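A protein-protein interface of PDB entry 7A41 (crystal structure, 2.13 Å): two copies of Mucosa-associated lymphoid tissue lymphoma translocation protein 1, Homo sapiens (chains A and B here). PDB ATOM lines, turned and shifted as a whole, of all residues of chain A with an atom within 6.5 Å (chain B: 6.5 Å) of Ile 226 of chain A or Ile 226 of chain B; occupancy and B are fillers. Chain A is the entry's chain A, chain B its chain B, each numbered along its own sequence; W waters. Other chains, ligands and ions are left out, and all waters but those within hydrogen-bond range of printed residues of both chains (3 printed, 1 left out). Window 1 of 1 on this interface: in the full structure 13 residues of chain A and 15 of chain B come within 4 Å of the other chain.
The side-chain carboxylate of Asp 206 of chain A is in hydrogen-bond range of the side-chain hydroxyl of Thr 202 of chain B, 2.8 Å away.
O of Ile 226 of chain A is in hydrogen-bond range of N of Ser 228 of chain B (2.8 Å).
OD1 of Asp 206 of chain B is in hydrogen-bond range of OG1 of Thr 202 of chain A (3.0 Å).
The guanidinium group (NH2) of Arg 227 of chain B lies close to the guanidinium group (NH2) of Arg 227 of chain A.
O of Ile 226 of chain B is in hydrogen-bond range of N of Ser 228 of chain A.
The backbone NH (N) of Phe 164 of chain B lies within hydrogen-bond range of the backbone carbonyl oxygen (O) of Arg 227 of chain B (2.7 Å).
The side-chain carboxylate (OE2) of Glu 225 of chain B is in salt-bridge range of the guanidinium group (NE) of Arg 227 of chain B (2.8 Å).
O of Glu 225 of chain B is in hydrogen-bond range of N of Tyr 166 of chain B (2.8 Å).
The side-chain carboxylate of Glu 225 of chain A lies within salt-bridge range of the guanidinium group of Arg 227 of chain A, 3.3 Å away.
N of Tyr 166 of chain A is in hydrogen-bond range of O of Glu 225 of chain A.
The backbone carbonyl oxygen (O) of Arg 227 of chain A sits at hydrogen-bond distance from the backbone NH (N) of Phe 164 of chain A (2.7 Å).
Leu 230 of chain B touches Ala 209 of chain A.
Leu 224 of chain A touches Ser 228 of chain B.
Ser 228 of chain B touches Glu 225 of chain A.
Ile 226 of chain A touches Ile 226 of chain B.
CA of Arg 227 of chain B touches O of Ile 226 of chain A (3.3 Å).
OE2 of Glu 225 of chain B touches CB of Arg 227 of chain A (3.5 Å).
Ile 226 of chain B touches Arg 227 of chain A (O to CA, 3.3 Å).
Leu 224 of chain B touches Ser 228 of chain A (O to O, 3.95 Å).
Ser 228 of chain A touches Glu 225 of chain B.
CA of Ser 229 of chain A touches O of Leu 224 of chain B, at 3.8 Å.
Ile 226 of chain A touches three residues of chain B.
Ile 226 of chain B touches just these residues of chain A: Ile 226 (3.6 Å), Arg 227 (3.3 Å) and Ser 228 (2.9 Å).
Of the printed residues of chain A, Leu 230 of chain B touches Ala 209.
Printed residues of chain B within 4 Å of Ala 209 of chain A: Leu 230 (3.9 Å).
Printed residues of chain A within 4 Å of Leu 224 of chain B: Ser 228 and Ser 229.
Printed residues of chain A within 4 Å of Asp 206 of chain B: Thr 202 (3.0 Å).
Of the printed residues of chain A, Ser 229 of chain B touches Leu 224 (3.5 Å).
The nearest printed residue of chain B that does not touch Ala 209 of chain A is Ser 229 of chain B (6.2 Å).
Of the 16 printed residues of chain A, 9 touch a printed residue of chain B.
Hydrophobic or aromatic side chains of chain A that line the printed part of chain B: Ala 209.
Of the 16 printed residues of chain B, 9 touch a printed residue of chain A.
Among the printed residues, no Asp or Glu carboxylate lies within 4 Å of a Lys or Arg side-chain nitrogen of the other chain.
Thr 202 of chain A touches Asp 206 of chain B, and with the chains exchanged Asp 206 of chain A touches Thr 202 of chain B.
Ala 209 of chain A touches Leu 230 of chain B, but with the chains exchanged Leu 230 of chain A does not touch Ala 209 of chain B (4.01 Å).
Leu 224 of chain A touches Ser 229 of chain B, and with the chains exchanged Ser 229 of chain A touches Leu 224 of chain B.
Glu 225 of chain A touches Ser 228 of chain B, and with the chains exchanged Ser 228 of chain A touches Glu 225 of chain B.
Positions printed for both chains: 163, 164, 165, 166, 202, 205, 206, 207, 209, 224, 225, 226, 227, 228, 229 and 230.
Of the 16 pairs that touch across the chains among the printed residues, 14 have their exchanged pair printed and touching as well.
Water W2 bridges O of Leu 230 of chain A (2.4 Å) and O of Asp 206 of chain B (3.1 Å).
Water W1 bridges the backbone carbonyl oxygen of Ser 228 of chain B and the backbone carbonyl oxygen of Leu 224 of chain A.
Water W3 lies within hydrogen-bond range of the side-chain hydroxyl of Ser 228 of chain B (3.1 Å), the backbone carbonyl oxygen of Leu 230 of chain B (3.2 Å) and the side-chain carboxylate of Asp 206 of chain A (3.2 Å).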
ATOM      1  N   VAL A 163      25.732  18.509   3.752  1.00  0.00           N
ATOM      2  CA  VAL A 163      24.368  18.803   3.335  1.00  0.00           C
ATOM      3  C   VAL A 163      23.561  18.872   4.630  1.00  0.00           C
ATOM      4  O   VAL A 163      23.543  17.918   5.418  1.00  0.00           O
ATOM      5  CB  VAL A 163      23.803  17.761   2.351  1.00  0.00           C
ATOM      6  CG1 VAL A 163      22.402  18.139   1.898  1.00  0.00           C
ATOM      7  CG2 VAL A 163      24.737  17.584   1.151  1.00  0.00           C
ATOM      8  N   PHE A 164      22.957  20.015   4.890  1.00  0.00           N
ATOM      9  CA  PHE A 164      22.204  20.246   6.109  1.00  0.00           C
ATOM     10  C   PHE A 164      20.736  20.543   5.779  1.00  0.00           C
ATOM     11  O   PHE A 164      20.434  21.358   4.921  1.00  0.00           O
ATOM     12  CB  PHE A 164      22.875  21.367   6.916  1.00  0.00           C
ATOM     13  CG  PHE A 164      22.087  21.958   8.065  1.00  0.00           C
ATOM     14  CD1 PHE A 164      22.042  21.325   9.291  1.00  0.00           C
ATOM     15  CD2 PHE A 164      21.457  23.188   7.937  1.00  0.00           C
ATOM     16  CE1 PHE A 164      21.344  21.879  10.352  1.00  0.00           C
ATOM     17  CE2 PHE A 164      20.785  23.761   9.019  1.00  0.00           C
ATOM     18  CZ  PHE A 164      20.716  23.093  10.215  1.00  0.00           C
ATOM     19  N   GLY A 165      19.843  19.793   6.384  1.00  0.00           N
ATOM     20  CA  GLY A 165      18.410  19.958   6.220  1.00  0.00           C
ATOM     21  C   GLY A 165      17.833  20.350   7.569  1.00  0.00           C
ATOM     22  O   GLY A 165      18.178  19.762   8.610  1.00  0.00           O
ATOM     23  N   TYR A 166      17.028  21.398   7.578  1.00  0.00           N
ATOM     24  CA  TYR A 166      16.461  21.935   8.801  1.00  0.00           C
ATOM     25  C   TYR A 166      14.958  22.127   8.596  1.00  0.00           C
ATOM     26  O   TYR A 166      14.504  23.064   7.927  1.00  0.00           O
ATOM     27  CB  TYR A 166      17.182  23.236   9.145  1.00  0.00           C
ATOM     28  CG  TYR A 166      16.778  23.917  10.430  1.00  0.00           C
ATOM     29  CD1 TYR A 166      16.157  23.214  11.451  1.00  0.00           C
ATOM     30  CD2 TYR A 166      17.081  25.249  10.655  1.00  0.00           C
ATOM     31  CE1 TYR A 166      15.803  23.836  12.642  1.00  0.00           C
ATOM     32  CE2 TYR A 166      16.731  25.880  11.839  1.00  0.00           C
ATOM     33  CZ  TYR A 166      16.097  25.170  12.834  1.00  0.00           C
ATOM     34  OH  TYR A 166      15.763  25.809  14.000  1.00  0.00           O
ATOM     35  N   THR A 202      21.380  16.522  -2.620  1.00  0.00           N
ATOM     36  CA  THR A 202      20.853  17.883  -2.719  1.00  0.00           C
ATOM     37  C   THR A 202      19.633  17.973  -3.621  1.00  0.00           C
ATOM     38  O   THR A 202      18.709  18.716  -3.295  1.00  0.00           O
ATOM     39  CB  THR A 202      21.923  18.849  -3.217  1.00  0.00           C
ATOM     40  OG1 THR A 202      22.515  18.313  -4.409  1.00  0.00           O
ATOM     41  CG2 THR A 202      22.977  19.129  -2.175  1.00  0.00           C
ATOM     42  N   LEU A 205      16.694  16.245  -1.770  1.00  0.00           N
ATOM     43  CA  LEU A 205      16.158  17.098  -0.700  1.00  0.00           C
ATOM     44  C   LEU A 205      15.376  18.286  -1.276  1.00  0.00           C
ATOM     45  O   LEU A 205      14.339  18.678  -0.724  1.00  0.00           O
ATOM     46  CB  LEU A 205      17.247  17.543   0.284  1.00  0.00           C
ATOM     47  CG  LEU A 205      17.836  16.413   1.106  1.00  0.00           C
ATOM     48  CD1 LEU A 205      18.993  16.893   1.912  1.00  0.00           C
ATOM     49  CD2 LEU A 205      16.777  15.778   2.009  1.00  0.00           C
ATOM     50  N   ASP A 206      15.817  18.787  -2.437  1.00  0.00           N
ATOM     51  CA  ASP A 206      15.124  19.836  -3.170  1.00  0.00           C
ATOM     52  C   ASP A 206      13.730  19.334  -3.589  1.00  0.00           C
ATOM     53  O   ASP A 206      12.770  20.094  -3.484  1.00  0.00           O
ATOM     54  CB  ASP A 206      15.930  20.241  -4.403  1.00  0.00           C
ATOM     55  CG  ASP A 206      15.306  21.385  -5.169  1.00  0.00           C
ATOM     56  OD1 ASP A 206      15.437  22.536  -4.714  1.00  0.00           O
ATOM     57  OD2 ASP A 206      14.670  21.122  -6.214  1.00  0.00           O
ATOM     58  N   GLU A 207      13.616  18.055  -4.050  1.00  0.00           N
ATOM     59  CA  GLU A 207      12.323  17.470  -4.416  1.00  0.00           C
ATOM     60  C   GLU A 207      11.437  17.380  -3.175  1.00  0.00           C
ATOM     61  O   GLU A 207      10.275  17.744  -3.243  1.00  0.00           O
ATOM     62  CB  GLU A 207      12.461  16.070  -5.019  1.00  0.00           C
ATOM     63  CG  GLU A 207      12.984  16.020  -6.438  1.00  0.00           C
ATOM     64  CD  GLU A 207      13.500  14.658  -6.858  1.00  0.00           C
ATOM     65  OE1 GLU A 207      13.773  14.487  -8.064  1.00  0.00           O
ATOM     66  OE2 GLU A 207      13.651  13.766  -5.991  1.00  0.00           O
ATOM     67  N   ALA A 209      11.471  19.352  -0.510  1.00  0.00           N
ATOM     68  CA  ALA A 209      10.999  20.711  -0.215  1.00  0.00           C
ATOM     69  C   ALA A 209       9.858  21.138  -1.148  1.00  0.00           C
ATOM     70  O   ALA A 209       8.918  21.805  -0.714  1.00  0.00           O
ATOM     71  CB  ALA A 209      12.152  21.701  -0.313  1.00  0.00           C
ATOM     72  N   LEU A 224      11.103  23.958   5.454  1.00  0.00           N
ATOM     73  CA  LEU A 224      12.338  23.235   5.175  1.00  0.00           C
ATOM     74  C   LEU A 224      13.415  24.155   4.622  1.00  0.00           C
ATOM     75  O   LEU A 224      13.186  24.883   3.651  1.00  0.00           O
ATOM     76  CB  LEU A 224      12.111  22.063   4.210  1.00  0.00           C
ATOM     77  CG  LEU A 224      13.344  21.199   3.930  1.00  0.00           C
ATOM     78  CD1 LEU A 224      13.894  20.569   5.195  1.00  0.00           C
ATOM     79  CD2 LEU A 224      13.048  20.134   2.938  1.00  0.00           C
ATOM     80  N   GLU A 225      14.591  24.129   5.241  1.00  0.00           N
ATOM     81  CA  GLU A 225      15.710  24.923   4.793  1.00  0.00           C
ATOM     82  C   GLU A 225      16.881  23.976   4.530  1.00  0.00           C
ATOM     83  O   GLU A 225      17.225  23.155   5.385  1.00  0.00           O
ATOM     84  CB  GLU A 225      16.093  25.970   5.845  1.00  0.00           C
ATOM     85  CG  GLU A 225      16.914  27.103   5.255  1.00  0.00           C
ATOM     86  CD  GLU A 225      17.978  27.698   6.158  1.00  0.00           C
ATOM     87  OE1 GLU A 225      18.045  27.300   7.344  1.00  0.00           O
ATOM     88  OE2 GLU A 225      18.751  28.557   5.675  1.00  0.00           O
ATOM     89  N   ILE A 226      17.486  24.080   3.349  1.00  0.00           N
ATOM     90  CA  ILE A 226      18.626  23.237   3.009  1.00  0.00           C
ATOM     91  C   ILE A 226      19.842  24.080   2.816  1.00  0.00           C
ATOM     92  O   ILE A 226      19.779  25.084   2.119  1.00  0.00           O
ATOM     93  CB  ILE A 226      18.345  22.387   1.745  1.00  0.00           C
ATOM     94  CG1 ILE A 226      17.019  21.622   1.854  1.00  0.00           C
ATOM     95  CG2 ILE A 226      19.507  21.439   1.438  1.00  0.00           C
ATOM     96  CD1 ILE A 226      16.452  21.303   0.477  1.00  0.00           C
ATOM     97  N   ARG A 227      20.949  23.702   3.435  1.00  0.00           N
ATOM     98  CA  ARG A 227      22.227  24.350   3.233  1.00  0.00           C
ATOM     99  C   ARG A 227      23.184  23.303   2.716  1.00  0.00           C
ATOM    100  O   ARG A 227      23.221  22.177   3.228  1.00  0.00           O
ATOM    101  CB  ARG A 227      22.773  24.958   4.516  1.00  0.00           C
ATOM    102  CG  ARG A 227      21.796  25.893   5.177  1.00  0.00           C
ATOM    103  CD  ARG A 227      22.393  26.421   6.441  1.00  0.00           C
ATOM    104  NE  ARG A 227      21.447  27.280   7.140  1.00  0.00           N
ATOM    105  CZ  ARG A 227      21.778  28.112   8.120  1.00  0.00           C
ATOM    106  NH1 ARG A 227      20.852  28.864   8.702  1.00  0.00           N
ATOM    107  NH2 ARG A 227      23.043  28.213   8.518  1.00  0.00           N
ATOM    108  N   SER A 228      23.979  23.669   1.723  1.00  0.00           N
ATOM    109  CA  SER A 228      24.920  22.733   1.156  1.00  0.00           C
ATOM    110  C   SER A 228      26.179  23.359   0.620  1.00  0.00           C
ATOM    111  O   SER A 228      26.156  24.356  -0.100  1.00  0.00           O
ATOM    112  CB  SER A 228      24.238  21.931   0.059  1.00  0.00           C
ATOM    113  OG  SER A 228      25.150  20.991  -0.480  1.00  0.00           O
ATOM    114  N   SER A 229      27.283  22.716   0.927  1.00  0.00           N
ATOM    115  CA  SER A 229      28.578  23.045   0.347  1.00  0.00           C
ATOM    116  C   SER A 229      29.052  21.785  -0.434  1.00  0.00           C
ATOM    117  O   SER A 229      30.239  21.496  -0.459  1.00  0.00           O
ATOM    118  CB  SER A 229      29.572  23.391   1.446  1.00  0.00           C
ATOM    119  OG  SER A 229      29.637  22.307   2.361  1.00  0.00           O
ATOM    120  N   LEU A 230      28.123  21.020  -1.041  1.00  0.00           N
ATOM    121  CA  LEU A 230      28.433  19.806  -1.776  1.00  0.00           C
ATOM    122  C   LEU A 230      28.868  20.193  -3.174  1.00  0.00           C
ATOM    123  O   LEU A 230      28.067  20.733  -3.943  1.00  0.00           O
ATOM    124  CB  LEU A 230      27.191  18.884  -1.835  1.00  0.00           C
ATOM    125  CG  LEU A 230      27.348  17.573  -2.630  1.00  0.00           C
ATOM    126  CD1 LEU A 230      28.481  16.734  -2.087  1.00  0.00           C
ATOM    127  CD2 LEU A 230      26.070  16.762  -2.611  1.00  0.00           C
ATOM    128  N   VAL B 163      16.678  32.004  -1.836  1.00  0.00           N
ATOM    129  CA  VAL B 163      17.786  31.192  -2.315  1.00  0.00           C
ATOM    130  C   VAL B 163      18.993  32.091  -2.156  1.00  0.00           C
ATOM    131  O   VAL B 163      19.070  33.168  -2.766  1.00  0.00           O
ATOM    132  CB  VAL B 163      17.647  30.744  -3.766  1.00  0.00           C
ATOM    133  CG1 VAL B 163      18.853  29.889  -4.173  1.00  0.00           C
ATOM    134  CG2 VAL B 163      16.334  30.000  -3.994  1.00  0.00           C
ATOM    135  N   PHE B 164      19.909  31.679  -1.297  1.00  0.00           N
ATOM    136  CA  PHE B 164      21.079  32.422  -0.927  1.00  0.00           C
ATOM    137  C   PHE B 164      22.361  31.700  -1.344  1.00  0.00           C
ATOM    138  O   PHE B 164      22.616  30.579  -0.934  1.00  0.00           O
ATOM    139  CB  PHE B 164      21.013  32.729   0.588  1.00  0.00           C
ATOM    140  CG  PHE B 164      22.266  33.259   1.248  1.00  0.00           C
ATOM    141  CD1 PHE B 164      22.794  34.483   0.886  1.00  0.00           C
ATOM    142  CD2 PHE B 164      22.881  32.556   2.271  1.00  0.00           C
ATOM    143  CE1 PHE B 164      23.917  34.981   1.512  1.00  0.00           C
ATOM    144  CE2 PHE B 164      24.020  33.044   2.882  1.00  0.00           C
ATOM    145  CZ  PHE B 164      24.523  34.260   2.516  1.00  0.00           C
ATOM    146  N   GLY B 165      23.142  32.356  -2.186  1.00  0.00           N
ATOM    147  CA  GLY B 165      24.416  31.843  -2.658  1.00  0.00           C
ATOM    148  C   GLY B 165      25.543  32.618  -2.017  1.00  0.00           C
ATOM    149  O   GLY B 165      25.664  33.828  -2.206  1.00  0.00           O
ATOM    150  N   TYR B 166      26.340  31.942  -1.216  1.00  0.00           N
ATOM    151  CA  TYR B 166      27.444  32.549  -0.506  1.00  0.00           C
ATOM    152  C   TYR B 166      28.749  32.040  -1.086  1.00  0.00           C
ATOM    153  O   TYR B 166      29.157  30.925  -0.798  1.00  0.00           O
ATOM    154  CB  TYR B 166      27.338  32.203   0.984  1.00  0.00           C
ATOM    155  CG  TYR B 166      28.369  32.863   1.866  1.00  0.00           C
ATOM    156  CD1 TYR B 166      28.915  34.092   1.531  1.00  0.00           C
ATOM    157  CD2 TYR B 166      28.750  32.291   3.069  1.00  0.00           C
ATOM    158  CE1 TYR B 166      29.858  34.705   2.340  1.00  0.00           C
ATOM    159  CE2 TYR B 166      29.680  32.904   3.895  1.00  0.00           C
ATOM    160  CZ  TYR B 166      30.235  34.109   3.525  1.00  0.00           C
ATOM    161  OH  TYR B 166      31.139  34.730   4.342  1.00  0.00           O
ATOM    162  N   THR B 202      17.585  26.687  -7.714  1.00  0.00           N
ATOM    163  CA  THR B 202      18.357  25.844  -6.784  1.00  0.00           C
ATOM    164  C   THR B 202      19.138  24.762  -7.537  1.00  0.00           C
ATOM    165  O   THR B 202      20.282  24.504  -7.212  1.00  0.00           O
ATOM    166  CB  THR B 202      17.425  25.215  -5.732  1.00  0.00           C
ATOM    167  OG1 THR B 202      16.325  24.598  -6.401  1.00  0.00           O
ATOM    168  CG2 THR B 202      16.886  26.240  -4.762  1.00  0.00           C
ATOM    169  N   LEU B 205      22.009  26.527  -9.498  1.00  0.00           N
ATOM    170  CA  LEU B 205      23.121  26.882  -8.610  1.00  0.00           C
ATOM    171  C   LEU B 205      23.896  25.637  -8.167  1.00  0.00           C
ATOM    172  O   LEU B 205      25.118  25.698  -8.054  1.00  0.00           O
ATOM    173  CB  LEU B 205      22.635  27.660  -7.394  1.00  0.00           C
ATOM    174  CG  LEU B 205      22.107  29.073  -7.663  1.00  0.00           C
ATOM    175  CD1 LEU B 205      21.696  29.705  -6.375  1.00  0.00           C
ATOM    176  CD2 LEU B 205      23.158  29.976  -8.338  1.00  0.00           C
ATOM    177  N   ASP B 206      23.195  24.510  -7.962  1.00  0.00           N
ATOM    178  CA  ASP B 206      23.793  23.225  -7.611  1.00  0.00           C
ATOM    179  C   ASP B 206      24.712  22.759  -8.757  1.00  0.00           C
ATOM    180  O   ASP B 206      25.776  22.212  -8.494  1.00  0.00           O
ATOM    181  CB  ASP B 206      22.700  22.171  -7.317  1.00  0.00           C
ATOM    182  CG  ASP B 206      23.290  20.833  -6.886  1.00  0.00           C
ATOM    183  OD1 ASP B 206      23.712  20.718  -5.699  1.00  0.00           O
ATOM    184  OD2 ASP B 206      23.365  19.909  -7.743  1.00  0.00           O
ATOM    185  N   GLU B 207      24.323  23.005 -10.025  1.00  0.00           N
ATOM    186  CA  GLU B 207      25.166  22.684 -11.184  1.00  0.00           C
ATOM    187  C   GLU B 207      26.388  23.611 -11.218  1.00  0.00           C
ATOM    188  O   GLU B 207      27.436  23.186 -11.682  1.00  0.00           O
ATOM    189  CB  GLU B 207      24.398  22.876 -12.504  1.00  0.00           C
ATOM    190  CG  GLU B 207      23.239  21.930 -12.732  1.00  0.00           C
ATOM    191  CD  GLU B 207      22.454  22.262 -13.984  1.00  0.00           C
ATOM    192  OE1 GLU B 207      22.049  21.323 -14.704  1.00  0.00           O
ATOM    193  OE2 GLU B 207      22.256  23.466 -14.258  1.00  0.00           O
ATOM    194  N   ALA B 209      27.869  24.923  -8.502  1.00  0.00           N
ATOM    195  CA  ALA B 209      28.685  24.371  -7.425  1.00  0.00           C
ATOM    196  C   ALA B 209      29.461  23.128  -7.889  1.00  0.00           C
ATOM    197  O   ALA B 209      30.631  22.958  -7.538  1.00  0.00           O
ATOM    198  CB  ALA B 209      27.812  24.021  -6.227  1.00  0.00           C
ATOM    199  N   LEU B 224      31.705  27.793  -2.253  1.00  0.00           N
ATOM    200  CA  LEU B 224      30.324  28.188  -2.481  1.00  0.00           C
ATOM    201  C   LEU B 224      29.359  27.405  -1.598  1.00  0.00           C
ATOM    202  O   LEU B 224      29.267  26.185  -1.715  1.00  0.00           O
ATOM    203  CB  LEU B 224      29.946  28.018  -3.981  1.00  0.00           C
ATOM    204  CG  LEU B 224      28.471  28.258  -4.349  1.00  0.00           C
ATOM    205  CD1 LEU B 224      28.068  29.734  -4.158  1.00  0.00           C
ATOM    206  CD2 LEU B 224      28.191  27.825  -5.771  1.00  0.00           C
ATOM    207  N   GLU B 225      28.617  28.106  -0.743  1.00  0.00           N
ATOM    208  CA  GLU B 225      27.568  27.478   0.039  1.00  0.00           C
ATOM    209  C   GLU B 225      26.209  27.960  -0.527  1.00  0.00           C
ATOM    210  O   GLU B 225      26.061  29.133  -0.871  1.00  0.00           O
ATOM    211  CB  GLU B 225      27.688  27.832   1.526  1.00  0.00           C
ATOM    212  CG  GLU B 225      26.568  27.201   2.335  1.00  0.00           C
ATOM    213  CD  GLU B 225      26.534  27.511   3.814  1.00  0.00           C
ATOM    214  OE1 GLU B 225      27.453  28.214   4.289  1.00  0.00           O
ATOM    215  OE2 GLU B 225      25.589  27.055   4.497  1.00  0.00           O
ATOM    216  N   ILE B 226      25.242  27.063  -0.658  1.00  0.00           N
ATOM    217  CA  ILE B 226      23.908  27.428  -1.118  1.00  0.00           C
ATOM    218  C   ILE B 226      22.947  27.162   0.020  1.00  0.00           C
ATOM    219  O   ILE B 226      22.911  26.044   0.519  1.00  0.00           O
ATOM    220  CB  ILE B 226      23.494  26.604  -2.355  1.00  0.00           C
ATOM    221  CG1 ILE B 226      24.532  26.712  -3.485  1.00  0.00           C
ATOM    222  CG2 ILE B 226      22.084  26.973  -2.812  1.00  0.00           C
ATOM    223  CD1 ILE B 226      24.390  25.595  -4.537  1.00  0.00           C
ATOM    224  N   ARG B 227      22.187  28.165   0.437  1.00  0.00           N
ATOM    225  CA  ARG B 227      21.171  28.019   1.467  1.00  0.00           C
ATOM    226  C   ARG B 227      19.812  28.328   0.814  1.00  0.00           C
ATOM    227  O   ARG B 227      19.689  29.335   0.121  1.00  0.00           O
ATOM    228  CB  ARG B 227      21.449  28.936   2.659  1.00  0.00           C
ATOM    229  CG  ARG B 227      22.867  28.803   3.192  1.00  0.00           C
ATOM    230  CD  ARG B 227      22.986  29.490   4.524  1.00  0.00           C
ATOM    231  NE  ARG B 227      24.372  29.553   4.996  1.00  0.00           N
ATOM    232  CZ  ARG B 227      24.750  30.162   6.116  1.00  0.00           C
ATOM    233  NH1 ARG B 227      26.029  30.200   6.457  1.00  0.00           N
ATOM    234  NH2 ARG B 227      23.851  30.741   6.903  1.00  0.00           N
ATOM    235  N   SER B 228      18.814  27.472   1.003  1.00  0.00           N
ATOM    236  CA  SER B 228      17.532  27.639   0.333  1.00  0.00           C
ATOM    237  C   SER B 228      16.299  27.222   1.129  1.00  0.00           C
ATOM    238  O   SER B 228      16.265  26.132   1.699  1.00  0.00           O
ATOM    239  CB  SER B 228      17.553  26.839  -0.968  1.00  0.00           C
ATOM    240  OG  SER B 228      16.283  26.771  -1.599  1.00  0.00           O
ATOM    241  N   SER B 229      15.236  28.026   1.044  1.00  0.00           N
ATOM    242  CA  SER B 229      13.933  27.642   1.596  1.00  0.00           C
ATOM    243  C   SER B 229      12.860  27.786   0.502  1.00  0.00           C
ATOM    244  O   SER B 229      11.699  28.010   0.811  1.00  0.00           O
ATOM    245  CB  SER B 229      13.576  28.447   2.837  1.00  0.00           C
ATOM    246  OG  SER B 229      13.344  29.801   2.492  1.00  0.00           O
ATOM    247  N   LEU B 230      13.251  27.630  -0.776  1.00  0.00           N
ATOM    248  CA  LEU B 230      12.389  27.689  -1.943  1.00  0.00           C
ATOM    249  C   LEU B 230      11.486  26.464  -1.886  1.00  0.00           C
ATOM    250  O   LEU B 230      11.983  25.353  -1.733  1.00  0.00           O
ATOM    251  CB  LEU B 230      13.272  27.660  -3.209  1.00  0.00           C
ATOM    252  CG  LEU B 230      12.577  27.638  -4.558  1.00  0.00           C
ATOM    253  CD1 LEU B 230      11.642  28.822  -4.715  1.00  0.00           C
ATOM    254  CD2 LEU B 230      13.585  27.605  -5.684  1.00  0.00           C
HETATM  255  O   HOH W   1      14.284  24.213   0.673  1.00  0.00           O
HETATM  256  O   HOH W   2      26.935  20.632  -6.064  1.00  0.00           O
HETATM  257  O   HOH W   3      14.846  24.006  -1.902  1.00  0.00           O
